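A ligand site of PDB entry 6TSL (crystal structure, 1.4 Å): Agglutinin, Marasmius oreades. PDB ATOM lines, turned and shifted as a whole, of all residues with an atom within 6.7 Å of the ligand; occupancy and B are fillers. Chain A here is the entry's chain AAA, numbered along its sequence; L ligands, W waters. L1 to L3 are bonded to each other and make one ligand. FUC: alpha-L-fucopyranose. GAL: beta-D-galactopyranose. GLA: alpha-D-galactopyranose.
OD1 of Asp 20 is in hydrogen-bond range of O6 of GAL L2 (2.6 Å). OD1 of Asn 43 lies within hydrogen-bond range of O2 of GLA L3. O3 of GLA L3 lies within hydrogen-bond range of N of Thr 38 (3.3 Å). An oxygen (O3) of GLA L3 lies within hydrogen-bond range of the side-chain hydroxyl (OG1) of Thr 38 (2.8 Å). O6 of GAL L2 is in hydrogen-bond range of N of Asp 23. An oxygen (O6) of GAL L2 lies within hydrogen-bond range of a ring nitrogen (ND1) of His 45 (3.0 Å). An oxygen (O5) of GLA L3 sits at hydrogen-bond distance from the indole nitrogen of Trp 35 (3.0 Å). O4 of GLA L3 lies within hydrogen-bond range of O of Gln 36.
OD2 of Asp 20 lies within hydrogen-bond range of NE2 of Gln 46, 2.9 Å away. The backbone carbonyl oxygen (O) of Asp 20 sits at hydrogen-bond distance from the backbone NH (N) of Val 33 (2.8 Å). The side-chain amide nitrogen (ND2) of Asn 43 sits at hydrogen-bond distance from the backbone carbonyl oxygen (O) of Thr 38, 3.1 Å away. ND2 of Asn 43 sits at hydrogen-bond distance from OG1 of Thr 41 (3.5 Å). The backbone carbonyl oxygen of Thr 38 is in hydrogen-bond range of the side-chain hydroxyl of Thr 41. A ring nitrogen (ND1) of His 45 is in hydrogen-bond range of the backbone NH of Gly 24. The backbone carbonyl oxygen (O) of Gln 36 lies within hydrogen-bond range of the side-chain amide nitrogen (NE2) of Gln 46, at 3.2 Å. The side-chain amide nitrogen of Gln 36 lies within hydrogen-bond range of the side-chain carboxylate of Asp 131, 2.9 Å away.
Merely in contact with the ligand: Leu 21 (3.6 Å), Lys 22 (3.6 Å), Phe 37 (3.7 Å) and Gln 46 (3.8 Å). 11 residues have an atom within 4 Å of the ligand: Asp 20, Leu 21, Lys 22, Asp 23, Trp 35, Gln 36, Phe 37, Thr 38, Asn 43, His 45 and Gln 46. The nearest printed residue that does not touch the ligand is Trp 44 (4.02 Å).
Water W1 lies within hydrogen-bond range of O3 of GLA L3, OG1 of Thr 41, O of Ile 42 and OD1 of Asn 43. Water W3 lies within hydrogen-bond range of O6 of GLA L3 (2.7 Å) and OD2 of Asp 131 (2.8 Å). Water W4 lies within hydrogen-bond range of an oxygen (O4) of GAL L2 (2.8 Å), the backbone NH (N) of His 45 (2.9 Å) and the backbone NH (N) of Trp 44 (3.2 Å). Water W7 lies within hydrogen-bond range of an oxygen (O2) of GLA L3, the backbone NH of Trp 44 and the backbone carbonyl oxygen of Ile 42.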
ATOM      1  N   HIS A   9     -28.900  13.722  20.860  1.00  0.00           N
ATOM      2  CA  HIS A   9     -27.864  13.293  19.912  1.00  0.00           C
ATOM      3  C   HIS A   9     -27.873  11.770  19.848  1.00  0.00           C
ATOM      4  O   HIS A   9     -27.704  11.156  20.894  1.00  0.00           O
ATOM      5  CB  HIS A   9     -26.518  13.852  20.345  1.00  0.00           C
ATOM      6  CG  HIS A   9     -25.451  13.735  19.311  1.00  0.00           C
ATOM      7  ND1 HIS A   9     -24.323  12.941  19.493  1.00  0.00           N
ATOM      8  CD2 HIS A   9     -25.351  14.249  18.056  1.00  0.00           C
ATOM      9  CE1 HIS A   9     -23.578  13.001  18.403  1.00  0.00           C
ATOM     10  NE2 HIS A   9     -24.177  13.826  17.532  1.00  0.00           N
ATOM     11  N   ASP A  20     -27.767  11.800  11.245  1.00  0.00           N
ATOM     12  CA  ASP A  20     -27.364  13.097  10.664  1.00  0.00           C
ATOM     13  C   ASP A  20     -28.312  13.419   9.496  1.00  0.00           C
ATOM     14  O   ASP A  20     -28.492  12.560   8.623  1.00  0.00           O
ATOM     15  CB  ASP A  20     -25.902  13.056  10.243  1.00  0.00           C
ATOM     16  CG  ASP A  20     -25.340  14.365   9.703  1.00  0.00           C
ATOM     17  OD1 ASP A  20     -25.808  14.795   8.621  1.00  0.00           O
ATOM     18  OD2 ASP A  20     -24.286  14.841  10.276  1.00  0.00           O
ATOM     19  N   LEU A  21     -28.946  14.580   9.506  1.00  0.00           N
ATOM     20  CA  LEU A  21     -29.712  15.053   8.324  1.00  0.00           C
ATOM     21  C   LEU A  21     -28.728  15.688   7.341  1.00  0.00           C
ATOM     22  O   LEU A  21     -28.116  16.727   7.711  1.00  0.00           O
ATOM     23  CB  LEU A  21     -30.770  16.057   8.766  1.00  0.00           C
ATOM     24  CG  LEU A  21     -31.641  16.601   7.633  1.00  0.00           C
ATOM     25  CD1 LEU A  21     -32.438  15.505   6.973  1.00  0.00           C
ATOM     26  CD2 LEU A  21     -32.581  17.687   8.150  1.00  0.00           C
ATOM     27  N   LYS A  22     -28.529  15.079   6.184  1.00  0.00           N
ATOM     28  CA  LYS A  22     -27.349  15.398   5.355  1.00  0.00           C
ATOM     29  C   LYS A  22     -27.375  16.903   4.971  1.00  0.00           C
ATOM     30  O   LYS A  22     -28.389  17.365   4.384  1.00  0.00           O
ATOM     31  CB  LYS A  22     -27.303  14.514   4.105  1.00  0.00           C
ATOM     32  CG  LYS A  22     -25.927  14.369   3.528  1.00  0.00           C
ATOM     33  CD  LYS A  22     -25.831  13.453   2.371  1.00  0.00           C
ATOM     34  CE  LYS A  22     -24.433  13.441   1.770  1.00  0.00           C
ATOM     35  NZ  LYS A  22     -24.240  12.273   0.874  1.00  0.00           N
ATOM     36  N   ASP A  23     -26.281  17.597   5.247  1.00  0.00           N
ATOM     37  CA  ASP A  23     -26.068  19.034   4.954  1.00  0.00           C
ATOM     38  C   ASP A  23     -27.129  19.893   5.684  1.00  0.00           C
ATOM     39  O   ASP A  23     -27.228  21.087   5.380  1.00  0.00           O
ATOM     40  CB  ASP A  23     -26.107  19.309   3.452  1.00  0.00           C
ATOM     41  CG  ASP A  23     -25.319  20.551   3.053  1.00  0.00           C
ATOM     42  OD1 ASP A  23     -24.294  20.831   3.710  1.00  0.00           O
ATOM     43  OD2 ASP A  23     -25.790  21.287   2.161  1.00  0.00           O
ATOM     44  N   GLY A  24     -27.854  19.307   6.628  1.00  0.00           N
ATOM     45  CA  GLY A  24     -28.882  20.035   7.385  1.00  0.00           C
ATOM     46  C   GLY A  24     -30.026  20.531   6.477  1.00  0.00           C
ATOM     47  O   GLY A  24     -30.739  21.448   6.895  1.00  0.00           O
ATOM     48  N   VAL A  33     -28.503   9.986   7.446  1.00  0.00           N
ATOM     49  CA  VAL A  33     -27.313   9.118   7.233  1.00  0.00           C
ATOM     50  C   VAL A  33     -26.554   8.987   8.555  1.00  0.00           C
ATOM     51  O   VAL A  33     -26.701   9.878   9.436  1.00  0.00           O
ATOM     52  CB  VAL A  33     -26.404   9.700   6.124  1.00  0.00           C
ATOM     53  CG1 VAL A  33     -27.098   9.685   4.772  1.00  0.00           C
ATOM     54  CG2 VAL A  33     -25.922  11.106   6.462  1.00  0.00           C
ATOM     55  N   TRP A  35     -23.011   9.547  10.463  1.00  0.00           N
ATOM     56  CA  TRP A  35     -21.899  10.532  10.325  1.00  0.00           C
ATOM     57  C   TRP A  35     -21.150  10.620  11.631  1.00  0.00           C
ATOM     58  O   TRP A  35     -21.799  10.580  12.679  1.00  0.00           O
ATOM     59  CB  TRP A  35     -22.443  11.914   9.890  1.00  0.00           C
ATOM     60  CG  TRP A  35     -21.460  12.739   9.113  1.00  0.00           C
ATOM     61  CD1 TRP A  35     -20.396  13.447   9.604  1.00  0.00           C
ATOM     62  CD2 TRP A  35     -21.437  12.915   7.682  1.00  0.00           C
ATOM     63  NE1 TRP A  35     -19.703  14.027   8.566  1.00  0.00           N
ATOM     64  CE2 TRP A  35     -20.319  13.726   7.390  1.00  0.00           C
ATOM     65  CE3 TRP A  35     -22.230  12.437   6.629  1.00  0.00           C
ATOM     66  CZ2 TRP A  35     -20.001  14.085   6.071  1.00  0.00           C
ATOM     67  CZ3 TRP A  35     -21.915  12.791   5.341  1.00  0.00           C
ATOM     68  CH2 TRP A  35     -20.816  13.606   5.064  1.00  0.00           C
ATOM     69  N   GLN A  36     -19.860  10.827  11.578  1.00  0.00           N
ATOM     70  CA  GLN A  36     -19.036  10.947  12.790  1.00  0.00           C
ATOM     71  C   GLN A  36     -19.342  12.281  13.487  1.00  0.00           C
ATOM     72  O   GLN A  36     -19.965  13.150  12.853  1.00  0.00           O
ATOM     73  CB  GLN A  36     -17.531  10.822  12.447  1.00  0.00           C
ATOM     74  CG  GLN A  36     -16.976  11.955  11.599  1.00  0.00           C
ATOM     75  CD  GLN A  36     -15.493  11.792  11.337  1.00  0.00           C
ATOM     76  OE1 GLN A  36     -14.678  11.815  12.262  1.00  0.00           O
ATOM     77  NE2 GLN A  36     -15.136  11.546  10.095  1.00  0.00           N
ATOM     78  N   PHE A  37     -18.928  12.419  14.722  1.00  0.00           N
ATOM     79  CA  PHE A  37     -19.313  13.579  15.552  1.00  0.00           C
ATOM     80  C   PHE A  37     -18.178  13.942  16.482  1.00  0.00           C
ATOM     81  O   PHE A  37     -17.221  13.165  16.615  1.00  0.00           O
ATOM     82  CB  PHE A  37     -20.597  13.252  16.320  1.00  0.00           C
ATOM     83  CG  PHE A  37     -20.530  12.032  17.200  1.00  0.00           C
ATOM     84  CD1 PHE A  37     -20.171  12.132  18.536  1.00  0.00           C
ATOM     85  CD2 PHE A  37     -20.943  10.787  16.732  1.00  0.00           C
ATOM     86  CE1 PHE A  37     -20.157  11.012  19.350  1.00  0.00           C
ATOM     87  CE2 PHE A  37     -20.959   9.678  17.557  1.00  0.00           C
ATOM     88  CZ  PHE A  37     -20.523   9.783  18.850  1.00  0.00           C
ATOM     89  N   THR A  38     -18.218  15.151  16.986  1.00  0.00           N
ATOM     90  CA  THR A  38     -17.253  15.660  17.977  1.00  0.00           C
ATOM     91  C   THR A  38     -17.987  15.886  19.280  1.00  0.00           C
ATOM     92  O   THR A  38     -18.856  16.739  19.353  1.00  0.00           O
ATOM     93  CB  THR A  38     -16.575  16.951  17.485  1.00  0.00           C
ATOM     94  OG1 THR A  38     -16.155  16.760  16.117  1.00  0.00           O
ATOM     95  CG2 THR A  38     -15.398  17.345  18.341  1.00  0.00           C
ATOM     96  N   PRO A  39     -17.688  15.105  20.331  1.00  0.00           N
ATOM     97  CA  PRO A  39     -18.260  15.367  21.660  1.00  0.00           C
ATOM     98  C   PRO A  39     -17.968  16.795  22.166  1.00  0.00           C
ATOM     99  O   PRO A  39     -16.966  17.389  21.732  1.00  0.00           O
ATOM    100  CB  PRO A  39     -17.588  14.307  22.561  1.00  0.00           C
ATOM    101  CG  PRO A  39     -17.288  13.153  21.604  1.00  0.00           C
ATOM    102  CD  PRO A  39     -16.957  13.829  20.281  1.00  0.00           C
ATOM    103  N   THR A  41     -19.325  19.589  21.487  1.00  0.00           N
ATOM    104  CA  THR A  41     -19.626  20.640  20.503  1.00  0.00           C
ATOM    105  C   THR A  41     -21.116  20.653  20.263  1.00  0.00           C
ATOM    106  O   THR A  41     -21.766  19.634  20.578  1.00  0.00           O
ATOM    107  CB  THR A  41     -18.866  20.415  19.168  1.00  0.00           C
ATOM    108  OG1 THR A  41     -19.451  19.304  18.475  1.00  0.00           O
ATOM    109  CG2 THR A  41     -17.398  20.176  19.352  1.00  0.00           C
ATOM    110  N   ILE A  42     -21.586  21.645  19.549  1.00  0.00           N
ATOM    111  CA  ILE A  42     -22.866  21.570  18.829  1.00  0.00           C
ATOM    112  C   ILE A  42     -22.646  20.799  17.528  1.00  0.00           C
ATOM    113  O   ILE A  42     -21.841  21.287  16.686  1.00  0.00           O
ATOM    114  CB  ILE A  42     -23.424  22.975  18.574  1.00  0.00           C
ATOM    115  CG1 ILE A  42     -23.713  23.706  19.891  1.00  0.00           C
ATOM    116  CG2 ILE A  42     -24.653  22.895  17.685  1.00  0.00           C
ATOM    117  CD1 ILE A  42     -24.705  23.009  20.775  1.00  0.00           C
ATOM    118  N   ASN A  43     -23.216  19.620  17.422  1.00  0.00           N
ATOM    119  CA  ASN A  43     -23.235  18.848  16.147  1.00  0.00           C
ATOM    120  C   ASN A  43     -24.456  19.269  15.332  1.00  0.00           C
ATOM    121  O   ASN A  43     -25.566  18.775  15.607  1.00  0.00           O
ATOM    122  CB  ASN A  43     -23.171  17.338  16.412  1.00  0.00           C
ATOM    123  CG  ASN A  43     -21.831  16.899  16.972  1.00  0.00           C
ATOM    124  OD1 ASN A  43     -20.844  16.812  16.246  1.00  0.00           O
ATOM    125  ND2 ASN A  43     -21.758  16.742  18.293  1.00  0.00           N
ATOM    126  N   TRP A  44     -24.272  20.260  14.463  1.00  0.00           N
ATOM    127  CA  TRP A  44     -25.341  21.146  13.947  1.00  0.00           C
ATOM    128  C   TRP A  44     -26.446  20.320  13.261  1.00  0.00           C
ATOM    129  O   TRP A  44     -27.567  20.778  13.255  1.00  0.00           O
ATOM    130  CB  TRP A  44     -24.746  22.188  13.005  1.00  0.00           C
ATOM    131  CG  TRP A  44     -24.141  23.333  13.715  1.00  0.00           C
ATOM    132  CD1 TRP A  44     -22.826  23.501  14.057  1.00  0.00           C
ATOM    133  CD2 TRP A  44     -24.854  24.436  14.292  1.00  0.00           C
ATOM    134  NE1 TRP A  44     -22.676  24.641  14.797  1.00  0.00           N
ATOM    135  CE2 TRP A  44     -23.888  25.245  14.922  1.00  0.00           C
ATOM    136  CE3 TRP A  44     -26.185  24.814  14.329  1.00  0.00           C
ATOM    137  CZ2 TRP A  44     -24.239  26.431  15.560  1.00  0.00           C
ATOM    138  CZ3 TRP A  44     -26.519  25.984  14.960  1.00  0.00           C
ATOM    139  CH2 TRP A  44     -25.563  26.759  15.599  1.00  0.00           C
ATOM    140  N   HIS A  45     -26.081  19.227  12.585  1.00  0.00           N
ATOM    141  CA  HIS A  45     -27.048  18.491  11.726  1.00  0.00           C
ATOM    142  C   HIS A  45     -27.558  17.232  12.437  1.00  0.00           C
ATOM    143  O   HIS A  45     -28.328  16.471  11.807  1.00  0.00           O
ATOM    144  CB  HIS A  45     -26.425  18.173  10.361  1.00  0.00           C
ATOM    145  CG  HIS A  45     -25.928  19.369   9.628  1.00  0.00           C
ATOM    146  ND1 HIS A  45     -24.981  19.273   8.600  1.00  0.00           N
ATOM    147  CD2 HIS A  45     -26.287  20.686   9.688  1.00  0.00           C
ATOM    148  CE1 HIS A  45     -24.734  20.497   8.111  1.00  0.00           C
ATOM    149  NE2 HIS A  45     -25.520  21.377   8.734  1.00  0.00           N
ATOM    150  N   GLN A  46     -27.250  17.077  13.719  1.00  0.00           N
ATOM    151  CA  GLN A  46     -27.357  15.755  14.416  1.00  0.00           C
ATOM    152  C   GLN A  46     -28.193  15.894  15.707  1.00  0.00           C
ATOM    153  O   GLN A  46     -28.064  15.015  16.566  1.00  0.00           O
ATOM    154  CB  GLN A  46     -25.976  15.205  14.730  1.00  0.00           C
ATOM    155  CG  GLN A  46     -25.091  15.059  13.504  1.00  0.00           C
ATOM    156  CD  GLN A  46     -23.740  14.461  13.803  1.00  0.00           C
ATOM    157  OE1 GLN A  46     -23.320  14.331  14.962  1.00  0.00           O
ATOM    158  NE2 GLN A  46     -22.989  14.187  12.732  1.00  0.00           N
ATOM    159  N   PHE A  66     -32.033  21.814  13.442  1.00  0.00           N
ATOM    160  CA  PHE A  66     -31.462  22.790  12.483  1.00  0.00           C
ATOM    161  C   PHE A  66     -32.483  23.047  11.346  1.00  0.00           C
ATOM    162  O   PHE A  66     -32.794  24.205  11.072  1.00  0.00           O
ATOM    163  CB  PHE A  66     -30.134  22.305  11.945  1.00  0.00           C
ATOM    164  CG  PHE A  66     -29.469  23.252  10.989  1.00  0.00           C
ATOM    165  CD1 PHE A  66     -28.784  24.367  11.457  1.00  0.00           C
ATOM    166  CD2 PHE A  66     -29.562  23.066   9.627  1.00  0.00           C
ATOM    167  CE1 PHE A  66     -28.173  25.239  10.569  1.00  0.00           C
ATOM    168  CE2 PHE A  66     -28.953  23.947   8.740  1.00  0.00           C
ATOM    169  CZ  PHE A  66     -28.269  25.030   9.222  1.00  0.00           C
ATOM    170  N   ASP A 131     -18.836   8.140   6.763  1.00  0.00           N
ATOM    171  CA  ASP A 131     -19.653   9.387   6.723  1.00  0.00           C
ATOM    172  C   ASP A 131     -20.586   9.332   5.523  1.00  0.00           C
ATOM    173  O   ASP A 131     -20.097   9.166   4.395  1.00  0.00           O
ATOM    174  CB  ASP A 131     -18.759  10.616   6.684  1.00  0.00           C
ATOM    175  CG  ASP A 131     -18.005  10.865   7.965  1.00  0.00           C
ATOM    176  OD1 ASP A 131     -18.451  10.332   9.036  1.00  0.00           O
ATOM    177  OD2 ASP A 131     -16.982  11.546   7.912  1.00  0.00           O
HETATM  178  C1  FUC L   1     -19.614  20.555  10.332  1.00  0.00           C
HETATM  179  C2  FUC L   1     -18.314  21.340  10.183  1.00  0.00           C
HETATM  180  C3  FUC L   1     -18.494  22.533   9.222  1.00  0.00           C
HETATM  181  C4  FUC L   1     -19.688  23.342   9.621  1.00  0.00           C
HETATM  182  C5  FUC L   1     -20.927  22.460   9.683  1.00  0.00           C
HETATM  183  C6  FUC L   1     -22.145  23.219  10.104  1.00  0.00           C
HETATM  184  O2  FUC L   1     -17.301  20.441   9.724  1.00  0.00           O
HETATM  185  O3  FUC L   1     -17.305  23.339   9.242  1.00  0.00           O
HETATM  186  O4  FUC L   1     -19.480  23.969  10.933  1.00  0.00           O
HETATM  187  O5  FUC L   1     -20.708  21.423  10.645  1.00  0.00           O
HETATM  188  C1  GAL L   2     -21.374  19.178   7.432  1.00  0.00           C
HETATM  189  C2  GAL L   2     -21.047  19.133   8.930  1.00  0.00           C
HETATM  190  C3  GAL L   2     -20.798  17.714   9.403  1.00  0.00           C
HETATM  191  C4  GAL L   2     -21.935  16.801   8.974  1.00  0.00           C
HETATM  192  C5  GAL L   2     -22.174  16.954   7.464  1.00  0.00           C
HETATM  193  C6  GAL L   2     -23.281  16.065   6.919  1.00  0.00           C
HETATM  194  O1  GAL L   2     -21.718  20.481   7.101  1.00  0.00           O
HETATM  195  O2  GAL L   2     -19.883  19.934   9.163  1.00  0.00           O
HETATM  196  O3  GAL L   2     -20.600  17.724  10.868  1.00  0.00           O
HETATM  197  O4  GAL L   2     -23.145  17.113   9.701  1.00  0.00           O
HETATM  198  O5  GAL L   2     -22.482  18.333   7.169  1.00  0.00           O
HETATM  199  O6  GAL L   2     -24.582  16.584   7.275  1.00  0.00           O
HETATM  200  C1  GLA L   3     -20.290  16.578  11.505  1.00  0.00           C
HETATM  201  C2  GLA L   3     -20.008  16.748  13.015  1.00  0.00           C
HETATM  202  C3  GLA L   3     -18.665  17.442  13.223  1.00  0.00           C
HETATM  203  C4  GLA L   3     -17.591  16.700  12.426  1.00  0.00           C
HETATM  204  C5  GLA L   3     -17.980  16.661  10.969  1.00  0.00           C
HETATM  205  C6  GLA L   3     -16.923  15.982  10.068  1.00  0.00           C
HETATM  206  O2  GLA L   3     -21.045  17.506  13.619  1.00  0.00           O
HETATM  207  O3  GLA L   3     -18.352  17.471  14.610  1.00  0.00           O
HETATM  208  O4  GLA L   3     -17.412  15.358  12.965  1.00  0.00           O
HETATM  209  O5  GLA L   3     -19.197  15.945  10.857  1.00  0.00           O
HETATM  210  O6  GLA L   3     -17.340  15.983   8.653  1.00  0.00           O
HETATM  211  O   HOH W   1     -19.412  19.683  15.707  1.00  0.00           O
HETATM  212  O   HOH W   2     -15.753  19.386  11.707  1.00  0.00           O
HETATM  213  O   HOH W   3     -16.537  14.081   6.888  1.00  0.00           O
HETATM  214  O   HOH W   4     -23.441  18.006  12.294  1.00  0.00           O
HETATM  215  O   HOH W   5     -17.416  18.555   7.617  1.00  0.00           O
HETATM  216  O   HOH W   6     -19.281  22.545  13.352  1.00  0.00           O
HETATM  217  O   HOH W   7     -21.273  20.441  13.575  1.00  0.00           O
